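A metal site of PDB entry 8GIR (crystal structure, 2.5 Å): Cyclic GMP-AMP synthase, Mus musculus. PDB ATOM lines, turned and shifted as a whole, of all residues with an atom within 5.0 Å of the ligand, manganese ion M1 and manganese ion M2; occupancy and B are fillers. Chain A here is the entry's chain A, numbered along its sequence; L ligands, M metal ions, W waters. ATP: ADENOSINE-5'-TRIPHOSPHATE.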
ATOM      1  N   GLY A  55     -13.597   8.064   6.604  1.00  0.00           N
ATOM      2  CA  GLY A  55     -14.956   7.567   6.631  1.00  0.00           C
ATOM      3  C   GLY A  55     -15.469   7.418   8.049  1.00  0.00           C
ATOM      4  O   GLY A  55     -14.796   7.730   9.035  1.00  0.00           O
ATOM      5  N   SER A  56     -16.705   6.921   8.132  1.00  0.00           N
ATOM      6  CA  SER A  56     -17.471   7.073   9.350  1.00  0.00           C
ATOM      7  C   SER A  56     -16.848   6.292  10.486  1.00  0.00           C
ATOM      8  O   SER A  56     -16.907   6.741  11.652  1.00  0.00           O
ATOM      9  CB  SER A  56     -18.920   6.641   9.129  1.00  0.00           C
ATOM     10  OG  SER A  56     -19.002   5.276   8.724  1.00  0.00           O
ATOM     11  N   GLU A  59     -14.124   8.333  11.955  1.00  0.00           N
ATOM     12  CA  GLU A  59     -14.733   9.527  12.542  1.00  0.00           C
ATOM     13  C   GLU A  59     -15.587   9.203  13.764  1.00  0.00           C
ATOM     14  O   GLU A  59     -16.069  10.132  14.436  1.00  0.00           O
ATOM     15  CB  GLU A  59     -15.570  10.277  11.484  1.00  0.00           C
ATOM     16  CG  GLU A  59     -14.774  10.838  10.295  1.00  0.00           C
ATOM     17  CD  GLU A  59     -15.630  11.041   9.055  1.00  0.00           C
ATOM     18  OE1 GLU A  59     -16.800  10.612   9.081  1.00  0.00           O
ATOM     19  OE2 GLU A  59     -15.172  11.637   8.042  1.00  0.00           O
ATOM     20  N   LYS A  62     -19.825   5.697  12.530  1.00  0.00           N
ATOM     21  CA  LYS A  62     -20.350   4.464  11.978  1.00  0.00           C
ATOM     22  C   LYS A  62     -21.428   3.914  12.903  1.00  0.00           C
ATOM     23  O   LYS A  62     -21.260   3.918  14.117  1.00  0.00           O
ATOM     24  CB  LYS A  62     -19.210   3.451  11.830  1.00  0.00           C
ATOM     25  CG  LYS A  62     -19.553   2.153  11.211  1.00  0.00           C
ATOM     26  CD  LYS A  62     -20.145   2.305   9.859  1.00  0.00           C
ATOM     27  CE  LYS A  62     -20.386   0.927   9.308  1.00  0.00           C
ATOM     28  NZ  LYS A  62     -21.811   0.642   9.058  1.00  0.00           N
ATOM     29  N   GLU A  68     -18.428  -1.653   7.529  1.00  0.00           N
ATOM     30  CA  GLU A  68     -18.000  -0.936   6.335  1.00  0.00           C
ATOM     31  C   GLU A  68     -16.883   0.020   6.712  1.00  0.00           C
ATOM     32  O   GLU A  68     -17.107   0.907   7.527  1.00  0.00           O
ATOM     33  CB  GLU A  68     -19.154  -0.189   5.694  1.00  0.00           C
ATOM     34  CG  GLU A  68     -18.995  -0.003   4.210  1.00  0.00           C
ATOM     35  CD  GLU A  68     -18.253   1.272   3.848  1.00  0.00           C
ATOM     36  OE1 GLU A  68     -17.937   2.044   4.747  1.00  0.00           O
ATOM     37  OE2 GLU A  68     -17.981   1.493   2.650  1.00  0.00           O
ATOM     38  N   ASP A  70     -13.464   2.475   5.267  1.00  0.00           N
ATOM     39  CA  ASP A  70     -12.935   3.171   4.089  1.00  0.00           C
ATOM     40  C   ASP A  70     -11.476   3.541   4.300  1.00  0.00           C
ATOM     41  O   ASP A  70     -11.121   4.095   5.350  1.00  0.00           O
ATOM     42  CB  ASP A  70     -13.747   4.422   3.754  1.00  0.00           C
ATOM     43  CG  ASP A  70     -15.218   4.169   3.761  1.00  0.00           C
ATOM     44  OD1 ASP A  70     -15.725   3.480   2.836  1.00  0.00           O
ATOM     45  OD2 ASP A  70     -15.876   4.643   4.699  1.00  0.00           O
ATOM     46  N   ASP A 164     -13.689  -0.415   1.362  1.00  0.00           N
ATOM     47  CA  ASP A 164     -13.417   0.309   0.139  1.00  0.00           C
ATOM     48  C   ASP A 164     -11.957   0.728   0.114  1.00  0.00           C
ATOM     49  O   ASP A 164     -11.534   1.521   0.958  1.00  0.00           O
ATOM     50  CB  ASP A 164     -14.299   1.560   0.051  1.00  0.00           C
ATOM     51  CG  ASP A 164     -15.747   1.230  -0.154  1.00  0.00           C
ATOM     52  OD1 ASP A 164     -16.069   0.089  -0.582  1.00  0.00           O
ATOM     53  OD2 ASP A 164     -16.571   2.113   0.120  1.00  0.00           O
ATOM     54  N   ARG A 221     -11.682  13.351  -9.482  1.00  0.00           N
ATOM     55  CA  ARG A 221     -12.573  14.091  -8.593  1.00  0.00           C
ATOM     56  C   ARG A 221     -11.865  14.413  -7.280  1.00  0.00           C
ATOM     57  O   ARG A 221     -11.218  13.535  -6.679  1.00  0.00           O
ATOM     58  CB  ARG A 221     -13.862  13.301  -8.314  1.00  0.00           C
ATOM     59  CG  ARG A 221     -14.933  14.073  -7.560  1.00  0.00           C
ATOM     60  CD  ARG A 221     -15.821  13.123  -6.750  1.00  0.00           C
ATOM     61  NE  ARG A 221     -15.249  12.937  -5.420  1.00  0.00           N
ATOM     62  CZ  ARG A 221     -15.287  11.795  -4.735  1.00  0.00           C
ATOM     63  NH1 ARG A 221     -15.879  10.713  -5.216  1.00  0.00           N
ATOM     64  NH2 ARG A 221     -14.713  11.747  -3.527  1.00  0.00           N
ATOM     65  N   PHE A 224     -11.842  15.357  -0.043  1.00  0.00           N
ATOM     66  CA  PHE A 224     -11.457  16.005   1.210  1.00  0.00           C
ATOM     67  C   PHE A 224     -11.768  15.120   2.406  1.00  0.00           C
ATOM     68  O   PHE A 224     -12.081  15.619   3.487  1.00  0.00           O
ATOM     69  CB  PHE A 224     -12.150  17.367   1.313  1.00  0.00           C
ATOM     70  CG  PHE A 224     -11.686  18.337   0.273  1.00  0.00           C
ATOM     71  CD1 PHE A 224     -10.489  19.011   0.436  1.00  0.00           C
ATOM     72  CD2 PHE A 224     -12.394  18.491  -0.890  1.00  0.00           C
ATOM     73  CE1 PHE A 224     -10.018  19.861  -0.527  1.00  0.00           C
ATOM     74  CE2 PHE A 224     -11.933  19.360  -1.888  1.00  0.00           C
ATOM     75  CZ  PHE A 224     -10.735  20.045  -1.711  1.00  0.00           C
ATOM     76  N   SER A 225     -11.695  13.793   2.223  1.00  0.00           N
ATOM     77  CA  SER A 225     -11.963  12.908   3.343  1.00  0.00           C
ATOM     78  C   SER A 225     -11.058  13.215   4.505  1.00  0.00           C
ATOM     79  O   SER A 225     -11.485  13.160   5.659  1.00  0.00           O
ATOM     80  CB  SER A 225     -11.790  11.449   2.954  1.00  0.00           C
ATOM     81  OG  SER A 225     -12.758  11.128   1.999  1.00  0.00           O
ATOM     82  N   GLU A 228     -12.422  16.234   6.298  1.00  0.00           N
ATOM     83  CA  GLU A 228     -13.635  15.886   7.010  1.00  0.00           C
ATOM     84  C   GLU A 228     -13.342  15.102   8.286  1.00  0.00           C
ATOM     85  O   GLU A 228     -13.980  15.312   9.324  1.00  0.00           O
ATOM     86  CB  GLU A 228     -14.574  15.126   6.072  1.00  0.00           C
ATOM     87  CG  GLU A 228     -14.891  15.958   4.821  1.00  0.00           C
ATOM     88  CD  GLU A 228     -15.502  15.124   3.724  1.00  0.00           C
ATOM     89  OE1 GLU A 228     -15.823  13.960   4.002  1.00  0.00           O
ATOM     90  OE2 GLU A 228     -15.688  15.630   2.597  1.00  0.00           O
ATOM     91  N   LYS A 259     -28.012   9.797   9.658  1.00  0.00           N
ATOM     92  CA  LYS A 259     -27.507   8.675   8.878  1.00  0.00           C
ATOM     93  C   LYS A 259     -28.474   7.517   8.933  1.00  0.00           C
ATOM     94  O   LYS A 259     -28.808   6.905   7.904  1.00  0.00           O
ATOM     95  CB  LYS A 259     -26.138   8.233   9.411  1.00  0.00           C
ATOM     96  CG  LYS A 259     -24.982   9.121   9.016  1.00  0.00           C
ATOM     97  CD  LYS A 259     -23.779   8.823   9.891  1.00  0.00           C
ATOM     98  CE  LYS A 259     -23.238   7.433   9.645  1.00  0.00           C
ATOM     99  NZ  LYS A 259     -22.656   7.361   8.306  1.00  0.00           N
ATOM    100  N   GLU A 263     -30.393   5.498   6.026  1.00  0.00           N
ATOM    101  CA  GLU A 263     -30.125   4.063   5.860  1.00  0.00           C
ATOM    102  C   GLU A 263     -31.402   3.225   5.860  1.00  0.00           C
ATOM    103  O   GLU A 263     -31.616   2.397   4.967  1.00  0.00           O
ATOM    104  CB  GLU A 263     -29.176   3.571   6.957  1.00  0.00           C
ATOM    105  CG  GLU A 263     -27.703   3.758   6.649  1.00  0.00           C
ATOM    106  CD  GLU A 263     -26.772   3.072   7.657  1.00  0.00           C
ATOM    107  OE1 GLU A 263     -27.162   2.000   8.185  1.00  0.00           O
ATOM    108  OE2 GLU A 263     -25.655   3.606   7.899  1.00  0.00           O
ATOM    109  N   CYS A 276     -27.218   9.226  -0.741  1.00  0.00           N
ATOM    110  CA  CYS A 276     -26.129   8.526  -0.080  1.00  0.00           C
ATOM    111  C   CYS A 276     -25.804   9.276   1.194  1.00  0.00           C
ATOM    112  O   CYS A 276     -26.165  10.442   1.364  1.00  0.00           O
ATOM    113  CB  CYS A 276     -24.901   8.401  -1.005  1.00  0.00           C
ATOM    114  SG  CYS A 276     -24.037   9.961  -1.313  1.00  0.00           S
ATOM    115  N   SER A 277     -25.066   8.618   2.072  1.00  0.00           N
ATOM    116  CA  SER A 277     -24.804   9.196   3.374  1.00  0.00           C
ATOM    117  C   SER A 277     -23.955  10.466   3.301  1.00  0.00           C
ATOM    118  O   SER A 277     -23.995  11.284   4.228  1.00  0.00           O
ATOM    119  CB  SER A 277     -24.113   8.153   4.239  1.00  0.00           C
ATOM    120  OG  SER A 277     -22.774   7.983   3.795  1.00  0.00           O
ATOM    121  N   TYR A 278     -23.197  10.681   2.229  1.00  0.00           N
ATOM    122  CA  TYR A 278     -22.437  11.919   2.121  1.00  0.00           C
ATOM    123  C   TYR A 278     -23.357  13.112   2.001  1.00  0.00           C
ATOM    124  O   TYR A 278     -22.956  14.233   2.342  1.00  0.00           O
ATOM    125  CB  TYR A 278     -21.498  11.877   0.921  1.00  0.00           C
ATOM    126  CG  TYR A 278     -20.481  12.996   0.877  1.00  0.00           C
ATOM    127  CD1 TYR A 278     -19.441  13.049   1.807  1.00  0.00           C
ATOM    128  CD2 TYR A 278     -20.537  14.011  -0.106  1.00  0.00           C
ATOM    129  CE1 TYR A 278     -18.481  14.074   1.776  1.00  0.00           C
ATOM    130  CE2 TYR A 278     -19.577  15.035  -0.137  1.00  0.00           C
ATOM    131  CZ  TYR A 278     -18.555  15.053   0.815  1.00  0.00           C
ATOM    132  OH  TYR A 278     -17.579  16.023   0.818  1.00  0.00           O
ATOM    133  N   LYS A 281     -23.999  14.007   5.556  1.00  0.00           N
ATOM    134  CA  LYS A 281     -22.761  14.550   6.118  1.00  0.00           C
ATOM    135  C   LYS A 281     -22.552  15.983   5.647  1.00  0.00           C
ATOM    136  O   LYS A 281     -22.196  16.860   6.453  1.00  0.00           O
ATOM    137  CB  LYS A 281     -21.564  13.692   5.714  1.00  0.00           C
ATOM    138  CG  LYS A 281     -20.262  14.039   6.409  1.00  0.00           C
ATOM    139  CD  LYS A 281     -19.107  13.252   5.828  1.00  0.00           C
ATOM    140  CE  LYS A 281     -17.983  13.064   6.859  1.00  0.00           C
ATOM    141  NZ  LYS A 281     -16.731  12.475   6.241  1.00  0.00           N
ATOM    142  N   HIS A 324     -21.809  21.430  -2.173  1.00  0.00           N
ATOM    143  CA  HIS A 324     -20.635  20.753  -1.646  1.00  0.00           C
ATOM    144  C   HIS A 324     -19.928  21.674  -0.661  1.00  0.00           C
ATOM    145  O   HIS A 324     -19.737  22.863  -0.941  1.00  0.00           O
ATOM    146  CB  HIS A 324     -19.722  20.382  -2.809  1.00  0.00           C
ATOM    147  CG  HIS A 324     -18.635  19.436  -2.462  1.00  0.00           C
ATOM    148  ND1 HIS A 324     -17.594  19.765  -1.607  1.00  0.00           N
ATOM    149  CD2 HIS A 324     -18.373  18.180  -2.884  1.00  0.00           C
ATOM    150  CE1 HIS A 324     -16.771  18.740  -1.499  1.00  0.00           C
ATOM    151  NE2 HIS A 324     -17.221  17.765  -2.266  1.00  0.00           N
HETATM  152  PG  ATP L   1     -21.146   5.354   6.015  1.00  0.00           P
HETATM  153  O1G ATP L   1     -22.475   5.479   5.322  1.00  0.00           O
HETATM  154  O2G ATP L   1     -21.218   4.939   7.465  1.00  0.00           O
HETATM  155  O3G ATP L   1     -20.241   4.411   5.246  1.00  0.00           O
HETATM  156  PB  ATP L   1     -19.098   7.388   5.301  1.00  0.00           P
HETATM  157  O1B ATP L   1     -18.903   8.842   5.452  1.00  0.00           O
HETATM  158  O2B ATP L   1     -17.914   6.526   5.649  1.00  0.00           O
HETATM  159  O3B ATP L   1     -20.344   6.739   6.017  1.00  0.00           O
HETATM  160  PA  ATP L   1     -18.864   6.306   2.562  1.00  0.00           P
HETATM  161  O1A ATP L   1     -19.938   6.307   1.549  1.00  0.00           O
HETATM  162  O2A ATP L   1     -18.380   5.004   3.170  1.00  0.00           O
HETATM  163  O3A ATP L   1     -19.475   7.104   3.779  1.00  0.00           O
HETATM  164  O5' ATP L   1     -17.655   7.134   1.968  1.00  0.00           O
HETATM  165  C5' ATP L   1     -16.438   7.332   2.719  1.00  0.00           C
HETATM  166  C4' ATP L   1     -15.970   8.766   2.593  1.00  0.00           C
HETATM  167  O4' ATP L   1     -15.688   9.087   1.214  1.00  0.00           O
HETATM  168  C3' ATP L   1     -16.930   9.858   3.053  1.00  0.00           C
HETATM  169  O3' ATP L   1     -16.807  10.067   4.456  1.00  0.00           O
HETATM  170  C2' ATP L   1     -16.421  11.073   2.272  1.00  0.00           C
HETATM  171  O2' ATP L   1     -15.232  11.620   2.835  1.00  0.00           O
HETATM  172  C1' ATP L   1     -16.037  10.436   0.941  1.00  0.00           C
HETATM  173  N9  ATP L   1     -17.126  10.433  -0.032  1.00  0.00           N
HETATM  174  C8  ATP L   1     -18.094   9.473  -0.218  1.00  0.00           C
HETATM  175  N7  ATP L   1     -18.959   9.757  -1.161  1.00  0.00           N
HETATM  176  C5  ATP L   1     -18.536  11.003  -1.622  1.00  0.00           C
HETATM  177  C6  ATP L   1     -19.020  11.855  -2.633  1.00  0.00           C
HETATM  178  N6  ATP L   1     -20.099  11.581  -3.388  1.00  0.00           N
HETATM  179  N1  ATP L   1     -18.351  13.008  -2.858  1.00  0.00           N
HETATM  180  C2  ATP L   1     -17.291  13.293  -2.103  1.00  0.00           C
HETATM  181  N3  ATP L   1     -16.747  12.580  -1.116  1.00  0.00           N
HETATM  182  C4  ATP L   1     -17.416  11.427  -0.935  1.00  0.00           C
HETATM  183 MN    MN M   1     -17.633   3.477   1.424  1.00  0.00          MN
HETATM  184 MN    MN M   2     -18.118   4.258   5.319  1.00  0.00          MN
HETATM  185  O   HOH W   1     -14.832  14.545   0.104  1.00  0.00           O
HETATM  186  O   HOH W   2     -21.050  10.071   4.546  1.00  0.00           O
HETATM  187  O   HOH W   3     -16.729   4.874  -0.146  1.00  0.00           O
HETATM  188  O   HOH W   4     -22.255   8.252   0.934  1.00  0.00           O
HETATM  189  O   HOH W   5     -18.952   9.883   7.915  1.00  0.00           O
HETATM  190  O   HOH W   6     -18.454  15.025  -4.968  1.00  0.00           O
HETATM  191  O   HOH W   7     -23.017   3.598   9.143  1.00  0.00           O
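Residues that only touch the ligand: Gly 55 (3.3 Å), Lys 62 (3.7 Å) and Tyr 278 (3.5 Å). Hydrophobic or aromatic side chains that line the ligand: Tyr 278.
The side-chain hydroxyl (OG) of Ser 277 lies within hydrogen-bond range of an oxygen (O1G) of the ligand (2.9 Å). NZ of Lys 259 lies within salt-bridge range of O2G of the ligand (2.9 Å). The side-chain amino group of Lys 281 sits at hydrogen-bond distance from an oxygen (O3') of the ligand, at 3.0 Å. The backbone NH (N) of Ser 56 lies close to an oxygen (O2B) of the ligand, at 2.8 Å. An oxygen (O2') of the ligand lies within hydrogen-bond range of the side-chain carboxylate (OE1) of Glu 228, at 2.7 Å. The side-chain hydroxyl (OG) of Ser 56 is in hydrogen-bond range of an oxygen (O2G) of the ligand. OG of Ser 225 sits at hydrogen-bond distance from O2' of the ligand, at 2.7 Å. N3 of the ligand lies within hydrogen-bond range of NH2 of Arg 221, 3.3 Å away.
Manganese ion M2 is bound by O3G of the ligand, O2A of the ligand, OE1 of Glu 68, O2B of the ligand and OD2 of Asp 70. Manganese ion M2 has five donor atoms within binding distance.
Water W2 lies within hydrogen-bond range of an oxygen (O1B) of the ligand (2.6 Å), the side-chain hydroxyl of Ser 277 (2.8 Å) and the backbone NH of Tyr 278 (3.2 Å). Water W5 lies within hydrogen-bond range of OE1 of Glu 59 (2.6 Å) and O1B of the ligand (2.7 Å). Water W7 lies within hydrogen-bond range of an oxygen (O2G) of the ligand (2.8 Å), the side-chain carboxylate of Glu 263 (2.9 Å) and the side-chain amino group of Lys 62 (3.2 Å). Water W1 lies within hydrogen-bond range of OE2 of Glu 228 (2.9 Å), N3 of the ligand (3.0 Å), N of Phe 224 (3.1 Å) and OH of Tyr 278 (3.2 Å). Water W4 lies within hydrogen-bond range of the backbone NH of Tyr 278 (2.9 Å), the side-chain hydroxyl of Ser 277 (2.9 Å), an oxygen (O1A) of the ligand (3.1 Å) and the side-chain sulfur of Cys 276 (3.3 Å).
Ser 56 touches manganese ion M2. Three residues have an atom within 4 Å of manganese ion M2: Ser 56, Glu 68 and Asp 70. Along chain A the residues within 4 Å of manganese ion M2 span positions 56 to 70.
Manganese ion M1 is bound by OD2 of Asp 164 (2.2 Å), water W3 (2.3 Å), OE2 of Glu 68 (2.4 Å), OD1 of Asp 70 (2.4 Å) and O2A of the ligand (2.4 Å). Manganese ion M1 has five donor atoms within binding distance.
Of the 18 residues printed, 3 come within 4 Å of manganese ion M1. The nearest printed residue that does not touch manganese ion M1 is Gly 55 (7.1 Å).
The side-chain amino group (NZ) of Lys 281 is in salt-bridge range of the side-chain carboxylate (OE1) of Glu 228, at 2.8 Å. The backbone carbonyl oxygen (O) of Ser 56 is in hydrogen-bond range of the backbone NH (N) of Lys 62. The backbone NH (N) of Tyr 278 sits close to the side-chain sulfur (SG) of Cys 276. NZ of Lys 281 lies within salt-bridge range of OE2 of Glu 59. The side-chain carboxylate of Glu 228 lies within hydrogen-bond range of the side-chain hydroxyl of Tyr 278 (2.6 Å).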
